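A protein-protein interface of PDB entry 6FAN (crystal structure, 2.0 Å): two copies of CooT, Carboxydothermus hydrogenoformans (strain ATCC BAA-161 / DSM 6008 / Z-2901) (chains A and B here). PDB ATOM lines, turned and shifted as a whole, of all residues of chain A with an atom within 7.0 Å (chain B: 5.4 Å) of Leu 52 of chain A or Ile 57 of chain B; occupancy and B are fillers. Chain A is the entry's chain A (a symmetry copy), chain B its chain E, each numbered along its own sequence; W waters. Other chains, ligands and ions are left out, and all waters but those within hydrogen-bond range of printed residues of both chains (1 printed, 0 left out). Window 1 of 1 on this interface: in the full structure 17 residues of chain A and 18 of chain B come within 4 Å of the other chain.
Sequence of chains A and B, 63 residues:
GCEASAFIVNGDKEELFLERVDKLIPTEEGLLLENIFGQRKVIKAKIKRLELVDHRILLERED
Cys 2 of chain A touches Leu 52 of chain B, and with the chains exchanged Leu 52 of chain A touches Cys 2 of chain B. Cys 2 of chain A touches His 55 of chain B, and with the chains exchanged His 55 of chain A touches Cys 2 of chain B. Ala 4 of chain A touches Leu 52 of chain B, and with the chains exchanged Leu 52 of chain A touches Ala 4 of chain B. Leu 52 of chain A touches Ile 57 of chain B, but with the chains exchanged Ile 57 of chain A does not touch Leu 52 of chain B (4.1 Å). Positions printed for both chains: 2, 3, 4, 50, 51, 52, 55, 56 and 57.
Of the printed residues of chain B, Leu 52 of chain A touches Cys 2, Ala 4, Val 21, Asp 22 and Ile 57. Ile 57 of chain B touches just one residue of chain A: Leu 52. Of the printed residues of chain A, Lys 23 of chain B touches Leu 50 and Glu 51. Printed residues of chain A within 4 Å of Val 21 of chain B: Leu 52. Of the printed residues of chain B, Leu 50 of chain A touches Asp 22 (3.7 Å), Lys 23 (3.3 Å) and Leu 24 (2.9 Å). Arg 56 of chain B touches none of the printed residues of chain A. The nearest residue of chain B that does not touch Leu 52 of chain A is Leu 52 of chain B (4.1 Å).
O of Cys 2 of chain A touches CB of Leu 52 of chain B (3.5 Å). ND1 of His 55 of chain B touches N of Cys 2 of chain A, at 3.7 Å. Leu 52 of chain B touches Ala 4 of chain A. Lys 23 of chain B touches Leu 50 of chain A (CA to O, 3.3 Å). Glu 51 of chain A touches Asp 22 of chain B (CA to O, 3.8 Å). CG of Glu 51 of chain A touches CD of Lys 23 of chain B, 3.9 Å away. O of Leu 52 of chain A touches N of Cys 2 of chain B (3.8 Å). Val 21 of chain B touches Leu 52 of chain A. Leu 52 of chain A touches Ile 57 of chain B. Val 53 of chain A touches Glu 3 of chain B.
Hydrophobic or aromatic side chains of chain A that line the printed part of chain B: Ala 4, Leu 50, Leu 52, Val 53 and His 55. Along chain A the printed residues that touch a printed residue of chain B span positions 2 to 55. Of the 20 printed residues of chain B, 10 touch a printed residue of chain A. Hydrophobic or aromatic side chains of chain B that line the printed part of chain A: Ala 4, Leu 24, Leu 52, His 55 and Ile 57. Among the printed residues, no Asp or Glu carboxylate lies within 4 Å of a Lys or Arg side-chain nitrogen of the other chain.
Water W1 lies within hydrogen-bond range of OD1 of Asp 22 of chain B (2.5 Å), N of Asp 54 of chain A (3.1 Å) and O of Glu 51 of chain A (3.4 Å).
The backbone NH (N) of Cys 2 of chain B sits close to the side-chain sulfur (SG) of Cys 2 of chain A (3.0 Å). O of Leu 24 of chain B sits at hydrogen-bond distance from N of Leu 50 of chain A (2.9 Å). The backbone carbonyl oxygen (O) of Asp 22 of chain B sits at hydrogen-bond distance from the backbone NH (N) of Leu 52 of chain A (2.9 Å). OD1 of Asp 22 of chain B lies within hydrogen-bond range of N of Val 53 of chain A (3.2 Å).
O of Glu 3 of chain A lies within hydrogen-bond range of ND1 of His 55 of chain A, 3.3 Å away. The guanidinium group of Arg 56 of chain A is in salt-bridge range of the side-chain carboxylate of Glu 51 of chain A (2.8 Å). The backbone NH of Val 21 of chain B is in hydrogen-bond range of the backbone carbonyl oxygen of Ala 4 of chain B (2.8 Å). The backbone NH of Ile 57 of chain B is in hydrogen-bond range of the backbone carbonyl oxygen of Ser 5 of chain B, 2.8 Å away. The backbone NH of Ser 5 of chain B is in hydrogen-bond range of the backbone carbonyl oxygen of His 55 of chain B (2.9 Å). The backbone NH (N) of Phe 7 of chain B sits at hydrogen-bond distance from the backbone carbonyl oxygen (O) of Ile 57 of chain B (2.8 Å).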
ATOM      1  N   CYS A   2      27.952  -1.790 -12.562  1.00  0.00           N
ATOM      2  CA  CYS A   2      28.934  -1.734 -13.679  1.00  0.00           C
ATOM      3  C   CYS A   2      29.225  -0.307 -14.188  1.00  0.00           C
ATOM      4  O   CYS A   2      28.426   0.658 -14.013  1.00  0.00           O
ATOM      5  CB  CYS A   2      28.515  -2.637 -14.853  1.00  0.00           C
ATOM      6  SG  CYS A   2      28.419  -4.314 -14.348  1.00  0.00           S
ATOM      7  N   GLU A   3      30.410  -0.166 -14.754  1.00  0.00           N
ATOM      8  CA  GLU A   3      30.837   1.022 -15.422  1.00  0.00           C
ATOM      9  C   GLU A   3      29.881   1.377 -16.585  1.00  0.00           C
ATOM     10  O   GLU A   3      29.348   0.527 -17.272  1.00  0.00           O
ATOM     11  CB  GLU A   3      32.278   0.846 -15.910  1.00  0.00           C
ATOM     12  CG  GLU A   3      32.541  -0.381 -16.796  1.00  0.00           C
ATOM     13  CD  GLU A   3      32.689  -1.696 -16.068  1.00  0.00           C
ATOM     14  OE1 GLU A   3      32.032  -2.003 -15.057  1.00  0.00           O
ATOM     15  OE2 GLU A   3      33.552  -2.477 -16.561  1.00  0.00           O
ATOM     16  N   ALA A   4      29.702   2.675 -16.780  1.00  0.00           N
ATOM     17  CA  ALA A   4      28.744   3.190 -17.754  1.00  0.00           C
ATOM     18  C   ALA A   4      29.416   4.134 -18.697  1.00  0.00           C
ATOM     19  O   ALA A   4      30.145   5.008 -18.260  1.00  0.00           O
ATOM     20  CB  ALA A   4      27.558   3.910 -16.988  1.00  0.00           C
ATOM     21  N   LEU A  50      20.551   8.720 -15.069  1.00  0.00           N
ATOM     22  CA  LEU A  50      21.391   7.512 -15.092  1.00  0.00           C
ATOM     23  C   LEU A  50      20.507   6.363 -15.522  1.00  0.00           C
ATOM     24  O   LEU A  50      19.366   6.259 -15.083  1.00  0.00           O
ATOM     25  CB  LEU A  50      21.953   7.211 -13.662  1.00  0.00           C
ATOM     26  CG  LEU A  50      22.658   8.290 -12.908  1.00  0.00           C
ATOM     27  CD1 LEU A  50      23.114   7.720 -11.555  1.00  0.00           C
ATOM     28  CD2 LEU A  50      23.826   8.846 -13.827  1.00  0.00           C
ATOM     29  N   GLU A  51      21.068   5.496 -16.345  1.00  0.00           N
ATOM     30  CA  GLU A  51      20.403   4.237 -16.746  1.00  0.00           C
ATOM     31  C   GLU A  51      21.433   3.170 -16.527  1.00  0.00           C
ATOM     32  O   GLU A  51      22.129   2.820 -17.441  1.00  0.00           O
ATOM     33  CB  GLU A  51      19.972   4.295 -18.208  1.00  0.00           C
ATOM     34  CG  GLU A  51      18.936   5.330 -18.509  1.00  0.00           C
ATOM     35  CD  GLU A  51      18.600   5.494 -19.967  1.00  0.00           C
ATOM     36  OE1 GLU A  51      19.365   5.018 -20.787  1.00  0.00           O
ATOM     37  OE2 GLU A  51      17.559   6.144 -20.220  1.00  0.00           O
ATOM     38  N   LEU A  52      21.516   2.671 -15.310  1.00  0.00           N
ATOM     39  CA  LEU A  52      22.651   1.834 -14.908  1.00  0.00           C
ATOM     40  C   LEU A  52      22.637   0.400 -15.446  1.00  0.00           C
ATOM     41  O   LEU A  52      23.706  -0.140 -15.757  1.00  0.00           O
ATOM     42  CB  LEU A  52      22.875   1.850 -13.411  1.00  0.00           C
ATOM     43  CG  LEU A  52      23.160   3.257 -12.814  1.00  0.00           C
ATOM     44  CD1 LEU A  52      23.445   3.127 -11.341  1.00  0.00           C
ATOM     45  CD2 LEU A  52      24.431   3.877 -13.459  1.00  0.00           C
ATOM     46  N   VAL A  53      21.444  -0.195 -15.578  1.00  0.00           N
ATOM     47  CA  VAL A  53      21.279  -1.498 -16.233  1.00  0.00           C
ATOM     48  C   VAL A  53      21.790  -1.397 -17.673  1.00  0.00           C
ATOM     49  O   VAL A  53      22.572  -2.261 -18.096  1.00  0.00           O
ATOM     50  CB  VAL A  53      19.797  -2.023 -16.183  1.00  0.00           C
ATOM     51  CG1 VAL A  53      19.639  -3.310 -17.018  1.00  0.00           C
ATOM     52  CG2 VAL A  53      19.421  -2.370 -14.769  1.00  0.00           C
ATOM     53  N   ASP A  54      21.441  -0.338 -18.369  1.00  0.00           N
ATOM     54  CA  ASP A  54      21.853  -0.094 -19.750  1.00  0.00           C
ATOM     55  C   ASP A  54      23.213   0.577 -19.941  1.00  0.00           C
ATOM     56  O   ASP A  54      23.542   0.951 -21.068  1.00  0.00           O
ATOM     57  CB  ASP A  54      20.766   0.718 -20.482  1.00  0.00           C
ATOM     58  CG  ASP A  54      19.418   0.006 -20.520  1.00  0.00           C
ATOM     59  OD1 ASP A  54      19.385  -1.220 -20.380  1.00  0.00           O
ATOM     60  OD2 ASP A  54      18.410   0.701 -20.726  1.00  0.00           O
ATOM     61  N   HIS A  55      23.986   0.725 -18.853  1.00  0.00           N
ATOM     62  CA  HIS A  55      25.366   1.270 -18.907  1.00  0.00           C
ATOM     63  C   HIS A  55      25.429   2.691 -19.524  1.00  0.00           C
ATOM     64  O   HIS A  55      26.333   2.981 -20.289  1.00  0.00           O
ATOM     65  CB  HIS A  55      26.343   0.350 -19.630  1.00  0.00           C
ATOM     66  CG  HIS A  55      26.313  -1.074 -19.147  1.00  0.00           C
ATOM     67  ND1 HIS A  55      26.709  -1.435 -17.880  1.00  0.00           N
ATOM     68  CD2 HIS A  55      25.863  -2.206 -19.737  1.00  0.00           C
ATOM     69  CE1 HIS A  55      26.520  -2.739 -17.710  1.00  0.00           C
ATOM     70  NE2 HIS A  55      26.033  -3.232 -18.831  1.00  0.00           N
ATOM     71  N   ARG A  56      24.482   3.569 -19.142  1.00  0.00           N
ATOM     72  CA  ARG A  56      24.416   4.907 -19.690  1.00  0.00           C
ATOM     73  C   ARG A  56      24.354   6.027 -18.615  1.00  0.00           C
ATOM     74  O   ARG A  56      23.563   5.947 -17.668  1.00  0.00           O
ATOM     75  CB  ARG A  56      23.206   5.047 -20.617  1.00  0.00           C
ATOM     76  CG  ARG A  56      23.329   4.205 -21.908  1.00  0.00           C
ATOM     77  CD  ARG A  56      22.016   3.910 -22.623  1.00  0.00           C
ATOM     78  NE  ARG A  56      21.161   5.053 -22.969  1.00  0.00           N
ATOM     79  CZ  ARG A  56      21.376   5.943 -23.959  1.00  0.00           C
ATOM     80  NH1 ARG A  56      22.430   5.885 -24.733  1.00  0.00           N
ATOM     81  NH2 ARG A  56      20.487   6.909 -24.166  1.00  0.00           N
ATOM     82  N   ILE A  57      25.156   7.065 -18.783  1.00  0.00           N
ATOM     83  CA  ILE A  57      25.073   8.270 -17.986  1.00  0.00           C
ATOM     84  C   ILE A  57      24.727   9.380 -18.967  1.00  0.00           C
ATOM     85  O   ILE A  57      25.518   9.656 -19.848  1.00  0.00           O
ATOM     86  CB  ILE A  57      26.438   8.613 -17.273  1.00  0.00           C
ATOM     87  CG1 ILE A  57      26.866   7.502 -16.309  1.00  0.00           C
ATOM     88  CG2 ILE A  57      26.331   9.953 -16.546  1.00  0.00           C
ATOM     89  CD1 ILE A  57      28.333   7.714 -15.880  1.00  0.00           C
ATOM     90  N   CYS B   2      25.620  -3.127 -14.361  1.00  0.00           N
ATOM     91  CA  CYS B   2      24.751  -3.565 -13.270  1.00  0.00           C
ATOM     92  C   CYS B   2      24.254  -2.426 -12.327  1.00  0.00           C
ATOM     93  O   CYS B   2      24.843  -1.342 -12.180  1.00  0.00           O
ATOM     94  CB  CYS B   2      25.381  -4.725 -12.467  1.00  0.00           C
ATOM     95  SG  CYS B   2      24.834  -6.375 -13.004  1.00  0.00           S
ATOM     96  N   GLU B   3      23.138  -2.745 -11.718  1.00  0.00           N
ATOM     97  CA  GLU B   3      22.512  -1.977 -10.688  1.00  0.00           C
ATOM     98  C   GLU B   3      23.451  -1.757  -9.511  1.00  0.00           C
ATOM     99  O   GLU B   3      24.255  -2.599  -9.104  1.00  0.00           O
ATOM    100  CB  GLU B   3      21.229  -2.686 -10.226  1.00  0.00           C
ATOM    101  CG  GLU B   3      20.412  -3.606 -11.174  1.00  0.00           C
ATOM    102  CD  GLU B   3      21.076  -4.948 -11.389  1.00  0.00           C
ATOM    103  OE1 GLU B   3      21.221  -5.395 -12.545  1.00  0.00           O
ATOM    104  OE2 GLU B   3      21.353  -5.625 -10.377  1.00  0.00           O
ATOM    105  N   ALA B   4      23.376  -0.567  -8.926  1.00  0.00           N
ATOM    106  CA  ALA B   4      24.320  -0.109  -7.872  1.00  0.00           C
ATOM    107  C   ALA B   4      23.379   0.252  -6.693  1.00  0.00           C
ATOM    108  O   ALA B   4      22.178   0.557  -6.920  1.00  0.00           O
ATOM    109  CB  ALA B   4      24.944   1.143  -8.384  1.00  0.00           C
ATOM    110  N   SER B   5      23.916   0.160  -5.475  1.00  0.00           N
ATOM    111  CA  SER B   5      23.186   0.597  -4.322  1.00  0.00           C
ATOM    112  C   SER B   5      23.374   2.082  -4.052  1.00  0.00           C
ATOM    113  O   SER B   5      24.508   2.620  -4.136  1.00  0.00           O
ATOM    114  CB  SER B   5      23.652  -0.224  -3.114  1.00  0.00           C
ATOM    115  OG  SER B   5      23.217  -1.556  -3.287  1.00  0.00           O
ATOM    116  N   ALA B   6      22.259   2.769  -3.685  1.00  0.00           N
ATOM    117  CA  ALA B   6      22.359   4.177  -3.258  1.00  0.00           C
ATOM    118  C   ALA B   6      22.469   4.291  -1.731  1.00  0.00           C
ATOM    119  O   ALA B   6      21.709   3.647  -1.007  1.00  0.00           O
ATOM    120  CB  ALA B   6      21.142   4.928  -3.762  1.00  0.00           C
ATOM    121  N   PHE B   7      23.370   5.129  -1.270  1.00  0.00           N
ATOM    122  CA  PHE B   7      23.600   5.369   0.163  1.00  0.00           C
ATOM    123  C   PHE B   7      23.439   6.847   0.484  1.00  0.00           C
ATOM    124  O   PHE B   7      23.788   7.693  -0.355  1.00  0.00           O
ATOM    125  CB  PHE B   7      25.014   4.949   0.561  1.00  0.00           C
ATOM    126  CG  PHE B   7      25.286   3.486   0.391  1.00  0.00           C
ATOM    127  CD1 PHE B   7      25.110   2.587   1.485  1.00  0.00           C
ATOM    128  CD2 PHE B   7      25.694   2.939  -0.865  1.00  0.00           C
ATOM    129  CE1 PHE B   7      25.367   1.207   1.332  1.00  0.00           C
ATOM    130  CE2 PHE B   7      25.931   1.552  -0.983  1.00  0.00           C
ATOM    131  CZ  PHE B   7      25.777   0.708   0.114  1.00  0.00           C
ATOM    132  N   VAL B  21      19.566  -0.023  -7.831  1.00  0.00           N
ATOM    133  CA  VAL B  21      19.048   1.116  -8.563  1.00  0.00           C
ATOM    134  C   VAL B  21      19.366   0.954 -10.048  1.00  0.00           C
ATOM    135  O   VAL B  21      20.526   0.647 -10.444  1.00  0.00           O
ATOM    136  CB  VAL B  21      19.720   2.447  -8.084  1.00  0.00           C
ATOM    137  CG1 VAL B  21      19.175   3.675  -8.865  1.00  0.00           C
ATOM    138  CG2 VAL B  21      19.436   2.603  -6.570  1.00  0.00           C
ATOM    139  N   ASP B  22      18.332   1.117 -10.868  1.00  0.00           N
ATOM    140  CA  ASP B  22      18.510   1.149 -12.298  1.00  0.00           C
ATOM    141  C   ASP B  22      18.517   2.610 -12.750  1.00  0.00           C
ATOM    142  O   ASP B  22      19.556   3.100 -13.242  1.00  0.00           O
ATOM    143  CB  ASP B  22      17.406   0.354 -13.002  1.00  0.00           C
ATOM    144  CG  ASP B  22      17.506   0.442 -14.521  1.00  0.00           C
ATOM    145  OD1 ASP B  22      18.509   0.882 -15.100  1.00  0.00           O
ATOM    146  OD2 ASP B  22      16.536   0.118 -15.186  1.00  0.00           O
ATOM    147  N   LYS B  23      17.387   3.314 -12.574  1.00  0.00           N
ATOM    148  CA  LYS B  23      17.291   4.707 -13.036  1.00  0.00           C
ATOM    149  C   LYS B  23      17.448   5.688 -11.908  1.00  0.00           C
ATOM    150  O   LYS B  23      16.956   5.454 -10.792  1.00  0.00           O
ATOM    151  CB  LYS B  23      15.942   4.961 -13.754  1.00  0.00           C
ATOM    152  CG  LYS B  23      15.512   3.914 -14.771  1.00  0.00           C
ATOM    153  CD  LYS B  23      16.044   4.020 -16.199  1.00  0.00           C
ATOM    154  CE  LYS B  23      15.590   2.845 -17.047  1.00  0.00           C
ATOM    155  NZ  LYS B  23      14.184   3.175 -17.371  1.00  0.00           N
ATOM    156  N   LEU B  24      18.169   6.770 -12.187  1.00  0.00           N
ATOM    157  CA  LEU B  24      18.207   7.901 -11.243  1.00  0.00           C
ATOM    158  C   LEU B  24      17.928   9.180 -12.054  1.00  0.00           C
ATOM    159  O   LEU B  24      18.646   9.483 -12.994  1.00  0.00           O
ATOM    160  CB  LEU B  24      19.584   7.978 -10.539  1.00  0.00           C
ATOM    161  CG  LEU B  24      19.731   8.964  -9.375  1.00  0.00           C
ATOM    162  CD1 LEU B  24      20.829   8.552  -8.421  1.00  0.00           C
ATOM    163  CD2 LEU B  24      20.004  10.373  -9.870  1.00  0.00           C
ATOM    164  N   ILE B  47      23.961  14.289  -5.608  1.00  0.00           N
ATOM    165  CA  ILE B  47      24.959  13.229  -5.761  1.00  0.00           C
ATOM    166  C   ILE B  47      26.315  13.733  -5.260  1.00  0.00           C
ATOM    167  O   ILE B  47      26.864  14.679  -5.799  1.00  0.00           O
ATOM    168  CB  ILE B  47      25.068  12.760  -7.222  1.00  0.00           C
ATOM    169  CG1 ILE B  47      23.756  12.084  -7.639  1.00  0.00           C
ATOM    170  CG2 ILE B  47      26.318  11.858  -7.375  1.00  0.00           C
ATOM    171  CD1 ILE B  47      23.567  11.964  -9.130  1.00  0.00           C
ATOM    172  N   ARG B  49      28.952  11.473  -5.079  1.00  0.00           N
ATOM    173  CA  ARG B  49      29.752  10.765  -6.027  1.00  0.00           C
ATOM    174  C   ARG B  49      29.192   9.425  -6.469  1.00  0.00           C
ATOM    175  O   ARG B  49      28.463   8.783  -5.756  1.00  0.00           O
ATOM    176  CB  ARG B  49      31.178  10.566  -5.510  1.00  0.00           C
ATOM    177  CG  ARG B  49      31.321   9.656  -4.310  1.00  0.00           C
ATOM    178  CD  ARG B  49      32.737   9.121  -4.109  1.00  0.00           C
ATOM    179  NE  ARG B  49      33.649  10.213  -3.972  1.00  0.00           N
ATOM    180  CZ  ARG B  49      34.913  10.205  -4.311  1.00  0.00           C
ATOM    181  NH1 ARG B  49      35.480   9.143  -4.773  1.00  0.00           N
ATOM    182  NH2 ARG B  49      35.599  11.289  -4.163  1.00  0.00           N
ATOM    183  N   LEU B  50      29.503   9.084  -7.699  1.00  0.00           N
ATOM    184  CA  LEU B  50      29.260   7.757  -8.238  1.00  0.00           C
ATOM    185  C   LEU B  50      30.546   6.989  -8.202  1.00  0.00           C
ATOM    186  O   LEU B  50      31.598   7.538  -8.546  1.00  0.00           O
ATOM    187  CB  LEU B  50      28.745   7.804  -9.693  1.00  0.00           C
ATOM    188  CG  LEU B  50      27.572   8.724 -10.045  1.00  0.00           C
ATOM    189  CD1 LEU B  50      27.173   8.400 -11.510  1.00  0.00           C
ATOM    190  CD2 LEU B  50      26.390   8.371  -9.107  1.00  0.00           C
ATOM    191  N   GLU B  51      30.478   5.729  -7.760  1.00  0.00           N
ATOM    192  CA  GLU B  51      31.617   4.830  -7.741  1.00  0.00           C
ATOM    193  C   GLU B  51      31.128   3.542  -8.352  1.00  0.00           C
ATOM    194  O   GLU B  51      30.721   2.630  -7.654  1.00  0.00           O
ATOM    195  CB  GLU B  51      32.083   4.576  -6.319  1.00  0.00           C
ATOM    196  CG  GLU B  51      32.622   5.806  -5.594  1.00  0.00           C
ATOM    197  CD  GLU B  51      32.990   5.479  -4.149  1.00  0.00           C
ATOM    198  OE1 GLU B  51      32.541   4.445  -3.641  1.00  0.00           O
ATOM    199  OE2 GLU B  51      33.703   6.243  -3.511  1.00  0.00           O
ATOM    200  N   LEU B  52      31.085   3.495  -9.681  1.00  0.00           N
ATOM    201  CA  LEU B  52      30.305   2.485 -10.386  1.00  0.00           C
ATOM    202  C   LEU B  52      30.935   1.084 -10.418  1.00  0.00           C
ATOM    203  O   LEU B  52      30.169   0.103 -10.406  1.00  0.00           O
ATOM    204  CB  LEU B  52      29.909   2.953 -11.760  1.00  0.00           C
ATOM    205  CG  LEU B  52      28.942   4.169 -11.752  1.00  0.00           C
ATOM    206  CD1 LEU B  52      28.635   4.568 -13.196  1.00  0.00           C
ATOM    207  CD2 LEU B  52      27.662   3.965 -10.880  1.00  0.00           C
ATOM    208  N   HIS B  55      29.840  -0.413  -7.264  1.00  0.00           N
ATOM    209  CA  HIS B  55      28.343  -0.484  -7.152  1.00  0.00           C
ATOM    210  C   HIS B  55      27.760   0.509  -6.182  1.00  0.00           C
ATOM    211  O   HIS B  55      26.864   0.154  -5.449  1.00  0.00           O
ATOM    212  CB  HIS B  55      27.873  -1.937  -6.824  1.00  0.00           C
ATOM    213  CG  HIS B  55      28.409  -2.975  -7.762  1.00  0.00           C
ATOM    214  ND1 HIS B  55      28.115  -2.993  -9.110  1.00  0.00           N
ATOM    215  CD2 HIS B  55      29.313  -3.960  -7.560  1.00  0.00           C
ATOM    216  CE1 HIS B  55      28.749  -4.003  -9.682  1.00  0.00           C
ATOM    217  NE2 HIS B  55      29.486  -4.605  -8.762  1.00  0.00           N
ATOM    218  N   ARG B  56      28.280   1.738  -6.158  1.00  0.00           N
ATOM    219  CA  ARG B  56      27.870   2.742  -5.137  1.00  0.00           C
ATOM    220  C   ARG B  56      27.407   4.077  -5.749  1.00  0.00           C
ATOM    221  O   ARG B  56      28.088   4.647  -6.602  1.00  0.00           O
ATOM    222  CB  ARG B  56      28.970   2.988  -4.119  1.00  0.00           C
ATOM    223  CG  ARG B  56      29.274   1.785  -3.264  1.00  0.00           C
ATOM    224  CD  ARG B  56      30.704   1.785  -2.628  1.00  0.00           C
ATOM    225  NE  ARG B  56      31.061   2.922  -1.803  1.00  0.00           N
ATOM    226  CZ  ARG B  56      30.599   3.149  -0.570  1.00  0.00           C
ATOM    227  NH1 ARG B  56      29.715   2.327   0.025  1.00  0.00           N
ATOM    228  NH2 ARG B  56      31.008   4.237   0.079  1.00  0.00           N
ATOM    229  N   ILE B  57      26.240   4.536  -5.279  1.00  0.00           N
ATOM    230  CA  ILE B  57      25.764   5.879  -5.590  1.00  0.00           C
ATOM    231  C   ILE B  57      25.720   6.578  -4.214  1.00  0.00           C
ATOM    232  O   ILE B  57      24.960   6.166  -3.359  1.00  0.00           O
ATOM    233  CB  ILE B  57      24.348   5.874  -6.212  1.00  0.00           C
ATOM    234  CG1 ILE B  57      24.337   5.120  -7.561  1.00  0.00           C
ATOM    235  CG2 ILE B  57      23.865   7.324  -6.389  1.00  0.00           C
ATOM    236  CD1 ILE B  57      22.909   4.644  -7.997  1.00  0.00           C
ATOM    237  N   LEU B  58      26.516   7.628  -4.015  1.00  0.00           N
ATOM    238  CA  LEU B  58      26.550   8.318  -2.735  1.00  0.00           C
ATOM    239  C   LEU B  58      25.851   9.642  -2.837  1.00  0.00           C
ATOM    240  O   LEU B  58      26.202  10.466  -3.668  1.00  0.00           O
ATOM    241  CB  LEU B  58      27.986   8.524  -2.229  1.00  0.00           C
ATOM    242  CG  LEU B  58      28.888   7.278  -2.229  1.00  0.00           C
ATOM    243  CD1 LEU B  58      30.151   7.704  -1.437  1.00  0.00           C
ATOM    244  CD2 LEU B  58      28.236   6.075  -1.547  1.00  0.00           C
ATOM    245  N   LEU B  59      24.852   9.790  -1.977  1.00  0.00           N
ATOM    246  CA  LEU B  59      23.955  10.934  -1.952  1.00  0.00           C
ATOM    247  C   LEU B  59      24.153  11.716  -0.651  1.00  0.00           C
ATOM    248  O   LEU B  59      24.496  11.129   0.381  1.00  0.00           O
ATOM    249  CB  LEU B  59      22.495  10.441  -2.045  1.00  0.00           C
ATOM    250  CG  LEU B  59      22.107   9.566  -3.237  1.00  0.00           C
ATOM    251  CD1 LEU B  59      20.667   9.098  -3.182  1.00  0.00           C
ATOM    252  CD2 LEU B  59      22.447  10.250  -4.546  1.00  0.00           C
HETATM  253  O   HOH W   1      18.979   1.424 -17.547  1.00  0.00           O
